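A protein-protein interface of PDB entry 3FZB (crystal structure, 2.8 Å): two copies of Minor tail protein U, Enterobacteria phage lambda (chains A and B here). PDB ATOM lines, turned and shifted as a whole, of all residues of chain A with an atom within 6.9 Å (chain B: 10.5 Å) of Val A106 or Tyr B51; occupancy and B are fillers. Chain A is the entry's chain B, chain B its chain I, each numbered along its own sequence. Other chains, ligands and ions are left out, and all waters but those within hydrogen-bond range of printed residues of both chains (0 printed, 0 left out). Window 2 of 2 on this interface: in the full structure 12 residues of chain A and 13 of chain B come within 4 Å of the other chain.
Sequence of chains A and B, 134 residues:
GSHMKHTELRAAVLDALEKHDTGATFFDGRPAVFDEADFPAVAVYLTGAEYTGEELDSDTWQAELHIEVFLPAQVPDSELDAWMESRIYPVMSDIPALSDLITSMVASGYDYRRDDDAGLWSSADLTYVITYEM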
ATOM      1  N   SER A 104     -33.782 -14.995 -36.032  1.00  0.00           N
ATOM      2  CA  SER A 104     -33.549 -15.805 -34.850  1.00  0.00           C
ATOM      3  C   SER A 104     -32.975 -14.919 -33.750  1.00  0.00           C
ATOM      4  O   SER A 104     -32.244 -13.970 -34.033  1.00  0.00           O
ATOM      5  CB  SER A 104     -32.599 -16.960 -35.167  1.00  0.00           C
ATOM      6  OG  SER A 104     -31.267 -16.505 -35.287  1.00  0.00           O
ATOM      7  N   MET A 105     -33.333 -15.213 -32.500  1.00  0.00           N
ATOM      8  CA  MET A 105     -32.843 -14.448 -31.348  1.00  0.00           C
ATOM      9  C   MET A 105     -32.563 -15.375 -30.167  1.00  0.00           C
ATOM     10  O   MET A 105     -33.309 -16.318 -29.895  1.00  0.00           O
ATOM     11  CB  MET A 105     -33.862 -13.370 -30.928  1.00  0.00           C
ATOM     12  CG  MET A 105     -33.408 -12.478 -29.763  1.00  0.00           C
ATOM     13  SD  MET A 105     -34.496 -11.065 -29.458  1.00  0.00           S
ATOM     14  CE  MET A 105     -33.337  -9.757 -29.421  1.00  0.00           C
ATOM     15  N   VAL A 106     -31.479 -15.109 -29.462  1.00  0.00           N
ATOM     16  CA  VAL A 106     -31.123 -15.934 -28.332  1.00  0.00           C
ATOM     17  C   VAL A 106     -30.273 -15.163 -27.341  1.00  0.00           C
ATOM     18  O   VAL A 106     -29.453 -14.304 -27.711  1.00  0.00           O
ATOM     19  CB  VAL A 106     -30.361 -17.194 -28.784  1.00  0.00           C
ATOM     20  CG1 VAL A 106     -29.146 -16.802 -29.610  1.00  0.00           C
ATOM     21  CG2 VAL A 106     -29.943 -18.006 -27.578  1.00  0.00           C
ATOM     22  N   ALA A 107     -30.500 -15.463 -26.068  1.00  0.00           N
ATOM     23  CA  ALA A 107     -29.760 -14.828 -25.003  1.00  0.00           C
ATOM     24  C   ALA A 107     -28.289 -15.026 -25.315  1.00  0.00           C
ATOM     25  O   ALA A 107     -27.883 -16.102 -25.773  1.00  0.00           O
ATOM     26  CB  ALA A 107     -30.100 -15.480 -23.697  1.00  0.00           C
ATOM     27  N   SER A 108     -27.502 -13.983 -25.088  1.00  0.00           N
ATOM     28  CA  SER A 108     -26.066 -14.041 -25.326  1.00  0.00           C
ATOM     29  C   SER A 108     -25.366 -13.949 -23.991  1.00  0.00           C
ATOM     30  O   SER A 108     -25.194 -14.945 -23.320  1.00  0.00           O
ATOM     31  CB  SER A 108     -25.616 -12.894 -26.213  1.00  0.00           C
ATOM     32  OG  SER A 108     -24.226 -12.990 -26.446  1.00  0.00           O
ATOM     33  N   GLY A 109     -24.980 -12.749 -23.590  1.00  0.00           N
ATOM     34  CA  GLY A 109     -24.325 -12.601 -22.304  1.00  0.00           C
ATOM     35  C   GLY A 109     -24.946 -11.562 -21.383  1.00  0.00           C
ATOM     36  O   GLY A 109     -26.073 -11.120 -21.597  1.00  0.00           O
ATOM     37  N   TYR A 110     -24.193 -11.180 -20.356  1.00  0.00           N
ATOM     38  CA  TYR A 110     -24.608 -10.184 -19.367  1.00  0.00           C
ATOM     39  C   TYR A 110     -23.305  -9.642 -18.782  1.00  0.00           C
ATOM     40  O   TYR A 110     -22.692 -10.278 -17.924  1.00  0.00           O
ATOM     41  CB  TYR A 110     -25.443 -10.856 -18.277  1.00  0.00           C
ATOM     42  CG  TYR A 110     -26.151  -9.898 -17.352  1.00  0.00           C
ATOM     43  CD1 TYR A 110     -27.548  -9.898 -17.258  1.00  0.00           C
ATOM     44  CD2 TYR A 110     -25.431  -8.978 -16.577  1.00  0.00           C
ATOM     45  CE1 TYR A 110     -28.207  -8.999 -16.422  1.00  0.00           C
ATOM     46  CE2 TYR A 110     -26.080  -8.086 -15.740  1.00  0.00           C
ATOM     47  CZ  TYR A 110     -27.467  -8.095 -15.671  1.00  0.00           C
ATOM     48  OH  TYR A 110     -28.111  -7.169 -14.891  1.00  0.00           O
ATOM     49  N   THR A 127     -27.085  -8.495 -23.653  1.00  0.00           N
ATOM     50  CA  THR A 127     -26.949  -8.727 -25.081  1.00  0.00           C
ATOM     51  C   THR A 127     -27.559 -10.027 -25.593  1.00  0.00           C
ATOM     52  O   THR A 127     -27.522 -11.059 -24.923  1.00  0.00           O
ATOM     53  CB  THR A 127     -25.464  -8.700 -25.482  1.00  0.00           C
ATOM     54  OG1 THR A 127     -24.751  -9.728 -24.771  1.00  0.00           O
ATOM     55  CG2 THR A 127     -24.862  -7.350 -25.151  1.00  0.00           C
ATOM     56  N   TYR A 128     -28.135  -9.956 -26.789  1.00  0.00           N
ATOM     57  CA  TYR A 128     -28.727 -11.125 -27.434  1.00  0.00           C
ATOM     58  C   TYR A 128     -27.995 -11.343 -28.759  1.00  0.00           C
ATOM     59  O   TYR A 128     -27.437 -10.402 -29.322  1.00  0.00           O
ATOM     60  CB  TYR A 128     -30.220 -10.907 -27.707  1.00  0.00           C
ATOM     61  CG  TYR A 128     -31.072 -10.729 -26.467  1.00  0.00           C
ATOM     62  CD1 TYR A 128     -31.056  -9.536 -25.746  1.00  0.00           C
ATOM     63  CD2 TYR A 128     -31.885 -11.765 -26.005  1.00  0.00           C
ATOM     64  CE1 TYR A 128     -31.828  -9.379 -24.599  1.00  0.00           C
ATOM     65  CE2 TYR A 128     -32.653 -11.619 -24.862  1.00  0.00           C
ATOM     66  CZ  TYR A 128     -32.620 -10.423 -24.166  1.00  0.00           C
ATOM     67  OH  TYR A 128     -33.384 -10.284 -23.038  1.00  0.00           O
ATOM     68  N   VAL A 129     -27.972 -12.579 -29.250  1.00  0.00           N
ATOM     69  CA  VAL A 129     -27.318 -12.848 -30.532  1.00  0.00           C
ATOM     70  C   VAL A 129     -28.419 -12.976 -31.565  1.00  0.00           C
ATOM     71  O   VAL A 129     -29.307 -13.807 -31.423  1.00  0.00           O
ATOM     72  CB  VAL A 129     -26.486 -14.152 -30.518  1.00  0.00           C
ATOM     73  CG1 VAL A 129     -25.852 -14.374 -31.884  1.00  0.00           C
ATOM     74  CG2 VAL A 129     -25.410 -14.066 -29.462  1.00  0.00           C
ATOM     75  N   ILE A 130     -28.369 -12.154 -32.605  1.00  0.00           N
ATOM     76  CA  ILE A 130     -29.410 -12.195 -33.625  1.00  0.00           C
ATOM     77  C   ILE A 130     -28.924 -12.535 -35.019  1.00  0.00           C
ATOM     78  O   ILE A 130     -27.727 -12.482 -35.304  1.00  0.00           O
ATOM     79  CB  ILE A 130     -30.143 -10.842 -33.711  1.00  0.00           C
ATOM     80  CG1 ILE A 130     -29.160  -9.740 -34.103  1.00  0.00           C
ATOM     81  CG2 ILE A 130     -30.810 -10.529 -32.371  1.00  0.00           C
ATOM     82  CD1 ILE A 130     -29.817  -8.441 -34.448  1.00  0.00           C
ATOM     83  N   HIS B   6     -27.280 -12.907 -10.098  1.00  0.00           N
ATOM     84  CA  HIS B   6     -25.906 -12.472  -9.939  1.00  0.00           C
ATOM     85  C   HIS B   6     -25.694 -11.717  -8.636  1.00  0.00           C
ATOM     86  O   HIS B   6     -24.592 -11.713  -8.084  1.00  0.00           O
ATOM     87  CB  HIS B   6     -25.500 -11.609 -11.119  1.00  0.00           C
ATOM     88  CG  HIS B   6     -25.430 -12.363 -12.409  1.00  0.00           C
ATOM     89  ND1 HIS B   6     -25.083 -11.769 -13.605  1.00  0.00           N
ATOM     90  CD2 HIS B   6     -25.660 -13.668 -12.688  1.00  0.00           C
ATOM     91  CE1 HIS B   6     -25.103 -12.679 -14.564  1.00  0.00           C
ATOM     92  NE2 HIS B   6     -25.450 -13.839 -14.033  1.00  0.00           N
ATOM     93  N   THR B  47     -17.311 -11.907 -14.655  1.00  0.00           N
ATOM     94  CA  THR B  47     -16.966 -11.509 -16.012  1.00  0.00           C
ATOM     95  C   THR B  47     -17.380 -12.658 -16.924  1.00  0.00           C
ATOM     96  O   THR B  47     -17.507 -13.807 -16.483  1.00  0.00           O
ATOM     97  CB  THR B  47     -15.462 -11.236 -16.205  1.00  0.00           C
ATOM     98  OG1 THR B  47     -14.713 -12.400 -15.849  1.00  0.00           O
ATOM     99  CG2 THR B  47     -15.017 -10.047 -15.374  1.00  0.00           C
ATOM    100  N   GLY B  48     -17.624 -12.341 -18.186  1.00  0.00           N
ATOM    101  CA  GLY B  48     -18.005 -13.360 -19.136  1.00  0.00           C
ATOM    102  C   GLY B  48     -19.235 -14.168 -18.801  1.00  0.00           C
ATOM    103  O   GLY B  48     -19.297 -15.344 -19.159  1.00  0.00           O
ATOM    104  N   ALA B  49     -20.208 -13.579 -18.111  1.00  0.00           N
ATOM    105  CA  ALA B  49     -21.439 -14.312 -17.810  1.00  0.00           C
ATOM    106  C   ALA B  49     -22.001 -14.574 -19.189  1.00  0.00           C
ATOM    107  O   ALA B  49     -21.946 -13.693 -20.038  1.00  0.00           O
ATOM    108  CB  ALA B  49     -22.392 -13.447 -17.027  1.00  0.00           C
ATOM    109  N   GLU B  50     -22.531 -15.761 -19.441  1.00  0.00           N
ATOM    110  CA  GLU B  50     -23.050 -16.023 -20.772  1.00  0.00           C
ATOM    111  C   GLU B  50     -23.972 -17.224 -20.850  1.00  0.00           C
ATOM    112  O   GLU B  50     -23.710 -18.265 -20.263  1.00  0.00           O
ATOM    113  CB  GLU B  50     -21.884 -16.203 -21.750  1.00  0.00           C
ATOM    114  CG  GLU B  50     -21.199 -17.559 -21.654  1.00  0.00           C
ATOM    115  CD  GLU B  50     -19.986 -17.681 -22.568  1.00  0.00           C
ATOM    116  OE1 GLU B  50     -20.081 -17.267 -23.747  1.00  0.00           O
ATOM    117  OE2 GLU B  50     -18.944 -18.206 -22.104  1.00  0.00           O
ATOM    118  N   TYR B  51     -25.056 -17.063 -21.591  1.00  0.00           N
ATOM    119  CA  TYR B  51     -26.040 -18.113 -21.778  1.00  0.00           C
ATOM    120  C   TYR B  51     -25.411 -19.327 -22.436  1.00  0.00           C
ATOM    121  O   TYR B  51     -24.531 -19.195 -23.281  1.00  0.00           O
ATOM    122  CB  TYR B  51     -27.171 -17.599 -22.656  1.00  0.00           C
ATOM    123  CG  TYR B  51     -28.298 -18.580 -22.806  1.00  0.00           C
ATOM    124  CD1 TYR B  51     -28.953 -19.087 -21.688  1.00  0.00           C
ATOM    125  CD2 TYR B  51     -28.721 -18.993 -24.060  1.00  0.00           C
ATOM    126  CE1 TYR B  51     -30.003 -19.975 -21.816  1.00  0.00           C
ATOM    127  CE2 TYR B  51     -29.770 -19.886 -24.197  1.00  0.00           C
ATOM    128  CZ  TYR B  51     -30.407 -20.370 -23.071  1.00  0.00           C
ATOM    129  OH  TYR B  51     -31.467 -21.233 -23.205  1.00  0.00           O
ATOM    130  N   THR B  52     -25.866 -20.514 -22.059  1.00  0.00           N
ATOM    131  CA  THR B  52     -25.302 -21.724 -22.636  1.00  0.00           C
ATOM    132  C   THR B  52     -26.307 -22.763 -23.127  1.00  0.00           C
ATOM    133  O   THR B  52     -25.931 -23.897 -23.410  1.00  0.00           O
ATOM    134  CB  THR B  52     -24.310 -22.401 -21.659  1.00  0.00           C
ATOM    135  OG1 THR B  52     -24.969 -22.707 -20.422  1.00  0.00           O
ATOM    136  CG2 THR B  52     -23.123 -21.485 -21.404  1.00  0.00           C
ATOM    137  N   GLY B  53     -27.578 -22.390 -23.233  1.00  0.00           N
ATOM    138  CA  GLY B  53     -28.553 -23.332 -23.745  1.00  0.00           C
ATOM    139  C   GLY B  53     -29.654 -23.775 -22.812  1.00  0.00           C
ATOM    140  O   GLY B  53     -29.678 -23.415 -21.635  1.00  0.00           O
ATOM    141  N   GLU B  54     -30.566 -24.580 -23.349  1.00  0.00           N
ATOM    142  CA  GLU B  54     -31.698 -25.087 -22.589  1.00  0.00           C
ATOM    143  C   GLU B  54     -31.535 -26.553 -22.202  1.00  0.00           C
ATOM    144  O   GLU B  54     -31.429 -27.431 -23.067  1.00  0.00           O
ATOM    145  CB  GLU B  54     -32.986 -24.900 -23.393  1.00  0.00           C
ATOM    146  N   GLU B  55     -31.517 -26.807 -20.894  1.00  0.00           N
ATOM    147  CA  GLU B  55     -31.398 -28.163 -20.362  1.00  0.00           C
ATOM    148  C   GLU B  55     -32.799 -28.724 -20.050  1.00  0.00           C
ATOM    149  O   GLU B  55     -32.962 -29.930 -19.866  1.00  0.00           O
ATOM    150  CB  GLU B  55     -30.518 -28.168 -19.100  1.00  0.00           C
ATOM    151  N   LEU B  56     -33.800 -27.842 -20.000  1.00  0.00           N
ATOM    152  CA  LEU B  56     -35.195 -28.224 -19.742  1.00  0.00           C
ATOM    153  C   LEU B  56     -36.047 -26.997 -19.419  1.00  0.00           C
ATOM    154  O   LEU B  56     -36.601 -26.869 -18.324  1.00  0.00           O
ATOM    155  CB  LEU B  56     -35.278 -29.230 -18.598  1.00  0.00           C
ATOM    156  N   SER B  58     -35.319 -24.880 -17.333  1.00  0.00           N
ATOM    157  CA  SER B  58     -33.934 -24.811 -16.870  1.00  0.00           C
ATOM    158  C   SER B  58     -33.013 -24.129 -17.897  1.00  0.00           C
ATOM    159  O   SER B  58     -32.689 -24.717 -18.929  1.00  0.00           O
ATOM    160  CB  SER B  58     -33.425 -26.226 -16.561  1.00  0.00           C
ATOM    161  N   ASP B  59     -32.591 -22.899 -17.604  1.00  0.00           N
ATOM    162  CA  ASP B  59     -31.705 -22.144 -18.501  1.00  0.00           C
ATOM    163  C   ASP B  59     -30.259 -22.034 -17.971  1.00  0.00           C
ATOM    164  O   ASP B  59     -29.992 -21.320 -17.002  1.00  0.00           O
ATOM    165  CB  ASP B  59     -32.290 -20.739 -18.749  1.00  0.00           C
ATOM    166  N   THR B  60     -29.331 -22.728 -18.626  1.00  0.00           N
ATOM    167  CA  THR B  60     -27.929 -22.732 -18.223  1.00  0.00           C
ATOM    168  C   THR B  60     -27.158 -21.453 -18.569  1.00  0.00           C
ATOM    169  O   THR B  60     -27.434 -20.789 -19.570  1.00  0.00           O
ATOM    170  CB  THR B  60     -27.231 -23.941 -18.835  1.00  0.00           C
ATOM    171  N   TRP B  61     -26.179 -21.126 -17.726  1.00  0.00           N
ATOM    172  CA  TRP B  61     -25.323 -19.952 -17.886  1.00  0.00           C
ATOM    173  C   TRP B  61     -23.926 -20.261 -17.374  1.00  0.00           C
ATOM    174  O   TRP B  61     -23.741 -21.111 -16.506  1.00  0.00           O
ATOM    175  CB  TRP B  61     -25.847 -18.779 -17.068  1.00  0.00           C
ATOM    176  CG  TRP B  61     -26.936 -18.011 -17.702  1.00  0.00           C
ATOM    177  CD1 TRP B  61     -28.244 -18.380 -17.827  1.00  0.00           C
ATOM    178  CD2 TRP B  61     -26.817 -16.731 -18.327  1.00  0.00           C
ATOM    179  NE1 TRP B  61     -28.949 -17.405 -18.497  1.00  0.00           N
ATOM    180  CE2 TRP B  61     -28.094 -16.383 -18.815  1.00  0.00           C
ATOM    181  CE3 TRP B  61     -25.752 -15.844 -18.526  1.00  0.00           C
ATOM    182  CZ2 TRP B  61     -28.332 -15.188 -19.489  1.00  0.00           C
ATOM    183  CZ3 TRP B  61     -25.990 -14.657 -19.198  1.00  0.00           C
ATOM    184  CH2 TRP B  61     -27.268 -14.341 -19.671  1.00  0.00           C
ATOM    185  N   GLN B  62     -22.935 -19.566 -17.906  1.00  0.00           N
ATOM    186  CA  GLN B  62     -21.567 -19.758 -17.447  1.00  0.00           C
ATOM    187  C   GLN B  62     -20.936 -18.396 -17.232  1.00  0.00           C
ATOM    188  O   GLN B  62     -21.100 -17.482 -18.041  1.00  0.00           O
ATOM    189  CB  GLN B  62     -20.736 -20.553 -18.450  1.00  0.00           C
ATOM    190  CG  GLN B  62     -19.324 -20.802 -17.958  1.00  0.00           C
ATOM    191  CD  GLN B  62     -18.578 -21.825 -18.799  1.00  0.00           C
ATOM    192  OE1 GLN B  62     -19.081 -22.927 -19.031  1.00  0.00           O
ATOM    193  NE2 GLN B  62     -17.366 -21.473 -19.244  1.00  0.00           N
ATOM    194  N   ALA B  63     -20.224 -18.256 -16.128  1.00  0.00           N
ATOM    195  CA  ALA B  63     -19.589 -16.995 -15.827  1.00  0.00           C
ATOM    196  C   ALA B  63     -18.256 -17.225 -15.158  1.00  0.00           C
ATOM    197  O   ALA B  63     -17.896 -18.353 -14.807  1.00  0.00           O
ATOM    198  CB  ALA B  63     -20.480 -16.169 -14.927  1.00  0.00           C
ATOM    199  N   GLU B  64     -17.529 -16.137 -14.979  1.00  0.00           N
ATOM    200  CA  GLU B  64     -16.242 -16.199 -14.339  1.00  0.00           C
ATOM    201  C   GLU B  64     -16.363 -15.425 -13.018  1.00  0.00           C
ATOM    202  O   GLU B  64     -16.670 -14.243 -13.011  1.00  0.00           O
ATOM    203  CB  GLU B  64     -15.209 -15.576 -15.270  1.00  0.00           C
ATOM    204  CG  GLU B  64     -13.798 -15.775 -14.812  1.00  0.00           C
ATOM    205  CD  GLU B  64     -12.991 -16.571 -15.795  1.00  0.00           C
ATOM    206  OE1 GLU B  64     -13.476 -17.650 -16.215  1.00  0.00           O
ATOM    207  OE2 GLU B  64     -11.871 -16.116 -16.135  1.00  0.00           O
ATOM    208  N   ILE B 130     -17.939 -20.672 -12.883  1.00  0.00           N
ATOM    209  CA  ILE B 130     -19.187 -21.185 -12.317  1.00  0.00           C
ATOM    210  C   ILE B 130     -20.322 -21.347 -13.317  1.00  0.00           C
ATOM    211  O   ILE B 130     -20.449 -20.560 -14.251  1.00  0.00           O
ATOM    212  CB  ILE B 130     -19.708 -20.298 -11.163  1.00  0.00           C
ATOM    213  CG1 ILE B 130     -19.984 -18.884 -11.663  1.00  0.00           C
ATOM    214  CG2 ILE B 130     -18.705 -20.285 -10.037  1.00  0.00           C
ATOM    215  N   THR B 131     -21.136 -22.380 -13.106  1.00  0.00           N
ATOM    216  CA  THR B 131     -22.295 -22.663 -13.946  1.00  0.00           C
ATOM    217  C   THR B 131     -23.530 -22.587 -13.059  1.00  0.00           C
ATOM    218  O   THR B 131     -23.488 -22.983 -11.897  1.00  0.00           O
ATOM    219  CB  THR B 131     -22.215 -24.062 -14.566  1.00  0.00           C
ATOM    220  OG1 THR B 131     -21.690 -24.978 -13.602  1.00  0.00           O
ATOM    221  CG2 THR B 131     -21.335 -24.050 -15.796  1.00  0.00           C
ATOM    222  N   TYR B 132     -24.639 -22.100 -13.605  1.00  0.00           N
ATOM    223  CA  TYR B 132     -25.844 -21.947 -12.804  1.00  0.00           C
ATOM    224  C   TYR B 132     -27.082 -21.703 -13.646  1.00  0.00           C
ATOM    225  O   TYR B 132     -26.995 -21.515 -14.860  1.00  0.00           O
ATOM    226  CB  TYR B 132     -25.648 -20.769 -11.853  1.00  0.00           C
ATOM    227  CG  TYR B 132     -25.208 -19.502 -12.566  1.00  0.00           C
ATOM    228  CD1 TYR B 132     -26.119 -18.487 -12.868  1.00  0.00           C
ATOM    229  CD2 TYR B 132     -23.879 -19.334 -12.970  1.00  0.00           C
ATOM    230  CE1 TYR B 132     -25.720 -17.335 -13.552  1.00  0.00           C
ATOM    231  CE2 TYR B 132     -23.468 -18.186 -13.661  1.00  0.00           C
ATOM    232  CZ  TYR B 132     -24.394 -17.192 -13.947  1.00  0.00           C
ATOM    233  OH  TYR B 132     -23.994 -16.070 -14.637  1.00  0.00           O
ATOM    234  N   GLU B 133     -28.235 -21.702 -12.984  1.00  0.00           N
ATOM    235  CA  GLU B 133     -29.511 -21.453 -13.641  1.00  0.00           C
ATOM    236  C   GLU B 133     -30.043 -20.057 -13.289  1.00  0.00           C
ATOM    237  O   GLU B 133     -30.079 -19.654 -12.123  1.00  0.00           O
ATOM    238  CB  GLU B 133     -30.526 -22.521 -13.243  1.00  0.00           C
ATOM    239  CG  GLU B 133     -30.404 -23.805 -14.041  1.00  0.00           C
ATOM    240  CD  GLU B 133     -31.266 -24.923 -13.484  1.00  0.00           C
ATOM    241  OE1 GLU B 133     -32.428 -24.652 -13.103  1.00  0.00           O
ATOM    242  OE2 GLU B 133     -30.781 -26.076 -13.437  1.00  0.00           O
ATOM    243  N   MET B 134     -30.450 -19.321 -14.314  1.00  0.00           N
ATOM    244  CA  MET B 134     -30.964 -17.974 -14.127  1.00  0.00           C
ATOM    245  C   MET B 134     -32.443 -18.045 -13.763  1.00  0.00           C
ATOM    246  O   MET B 134     -32.791 -17.600 -12.646  1.00  0.00           O
ATOM    247  CB  MET B 134     -30.773 -17.168 -15.413  1.00  0.00           C
ATOM    248  CG  MET B 134     -30.727 -15.664 -15.218  1.00  0.00           C
ATOM    249  SD  MET B 134     -29.209 -15.061 -14.448  1.00  0.00           S
ATOM    250  CE  MET B 134     -28.254 -14.576 -15.884  1.00  0.00           C
ATOM    251  OXT MET B 134     -33.227 -18.552 -14.598  1.00  0.00           O
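The backbone carbonyl oxygen (O) of Ser A108 is in hydrogen-bond range of the backbone NH (N) of Tyr B51 (2.7 Å). O of Ala B49 lies within hydrogen-bond range of N of Tyr A110 (3.4 Å).
The backbone NH (N) of Trp B61 sits at hydrogen-bond distance from the backbone carbonyl oxygen (O) of Tyr B132, at 3.0 Å. The side-chain hydroxyl of Tyr B51 lies within hydrogen-bond range of the backbone NH of Glu B54 (3.5 Å). N of Glu B50 lies within hydrogen-bond range of O of Gln B62 (2.6 Å). The side-chain hydroxyl (OG1) of Thr A127 is in hydrogen-bond range of the backbone NH (N) of Gly A109 (3.3 Å). O of Val A106 sits at hydrogen-bond distance from N of Val A129, at 2.7 Å. N of Trp B61 sits at hydrogen-bond distance from OG1 of Thr B52 (3.4 Å).
CG2 of Val A106 touches CD2 of Tyr B51, at 3.9 Å. Ala A107 touches Tyr B51. O of Ser A108 touches CA of Glu B50, at 3.5 Å. Gly A109 touches Ala B49 (CA to O, 3.5 Å). CA of Gly A109 touches CA of Glu B50 (3.96 Å). Trp B61 touches Gly A109. CB of Tyr A110 touches CZ3 of Trp B61 (3.9 Å).
No residue of chain B comes within 4 Å of Met A105. Of the printed residues of chain B, Val A106 touches Tyr B51. Ala A107 touches one residue of chain B. Ser A108 touches two residues of chain B. Printed residues of chain B within 4 Å of Tyr A110: Ala B49 and Trp B61. Val A129 touches none of the printed residues of chain B. Of the printed residues of chain A, Ala B49 touches Gly A109 (3.5 Å) and Tyr A110 (3.3 Å). Printed residues of chain A within 4 Å of Glu B50: Ser A108 (3.5 Å) and Gly A109 (3.96 Å). Tyr B51 touches three residues of chain A. Thr B60 touches none of the printed residues of chain A. The nearest residue of chain B that does not touch Val A106 is Gly B53 (6.6 Å). The nearest printed residue of chain B that does not touch Tyr A110 is His B6 (4.1 Å).
Of the 11 printed residues of chain A, 5 touch a printed residue of chain B. Hydrophobic or aromatic side chains of chain A that line the printed part of chain B: Val A106, Ala A107 and Tyr A110. Among the printed residues, 9 pairs touch across the chains.
1 position is printed for both chains.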
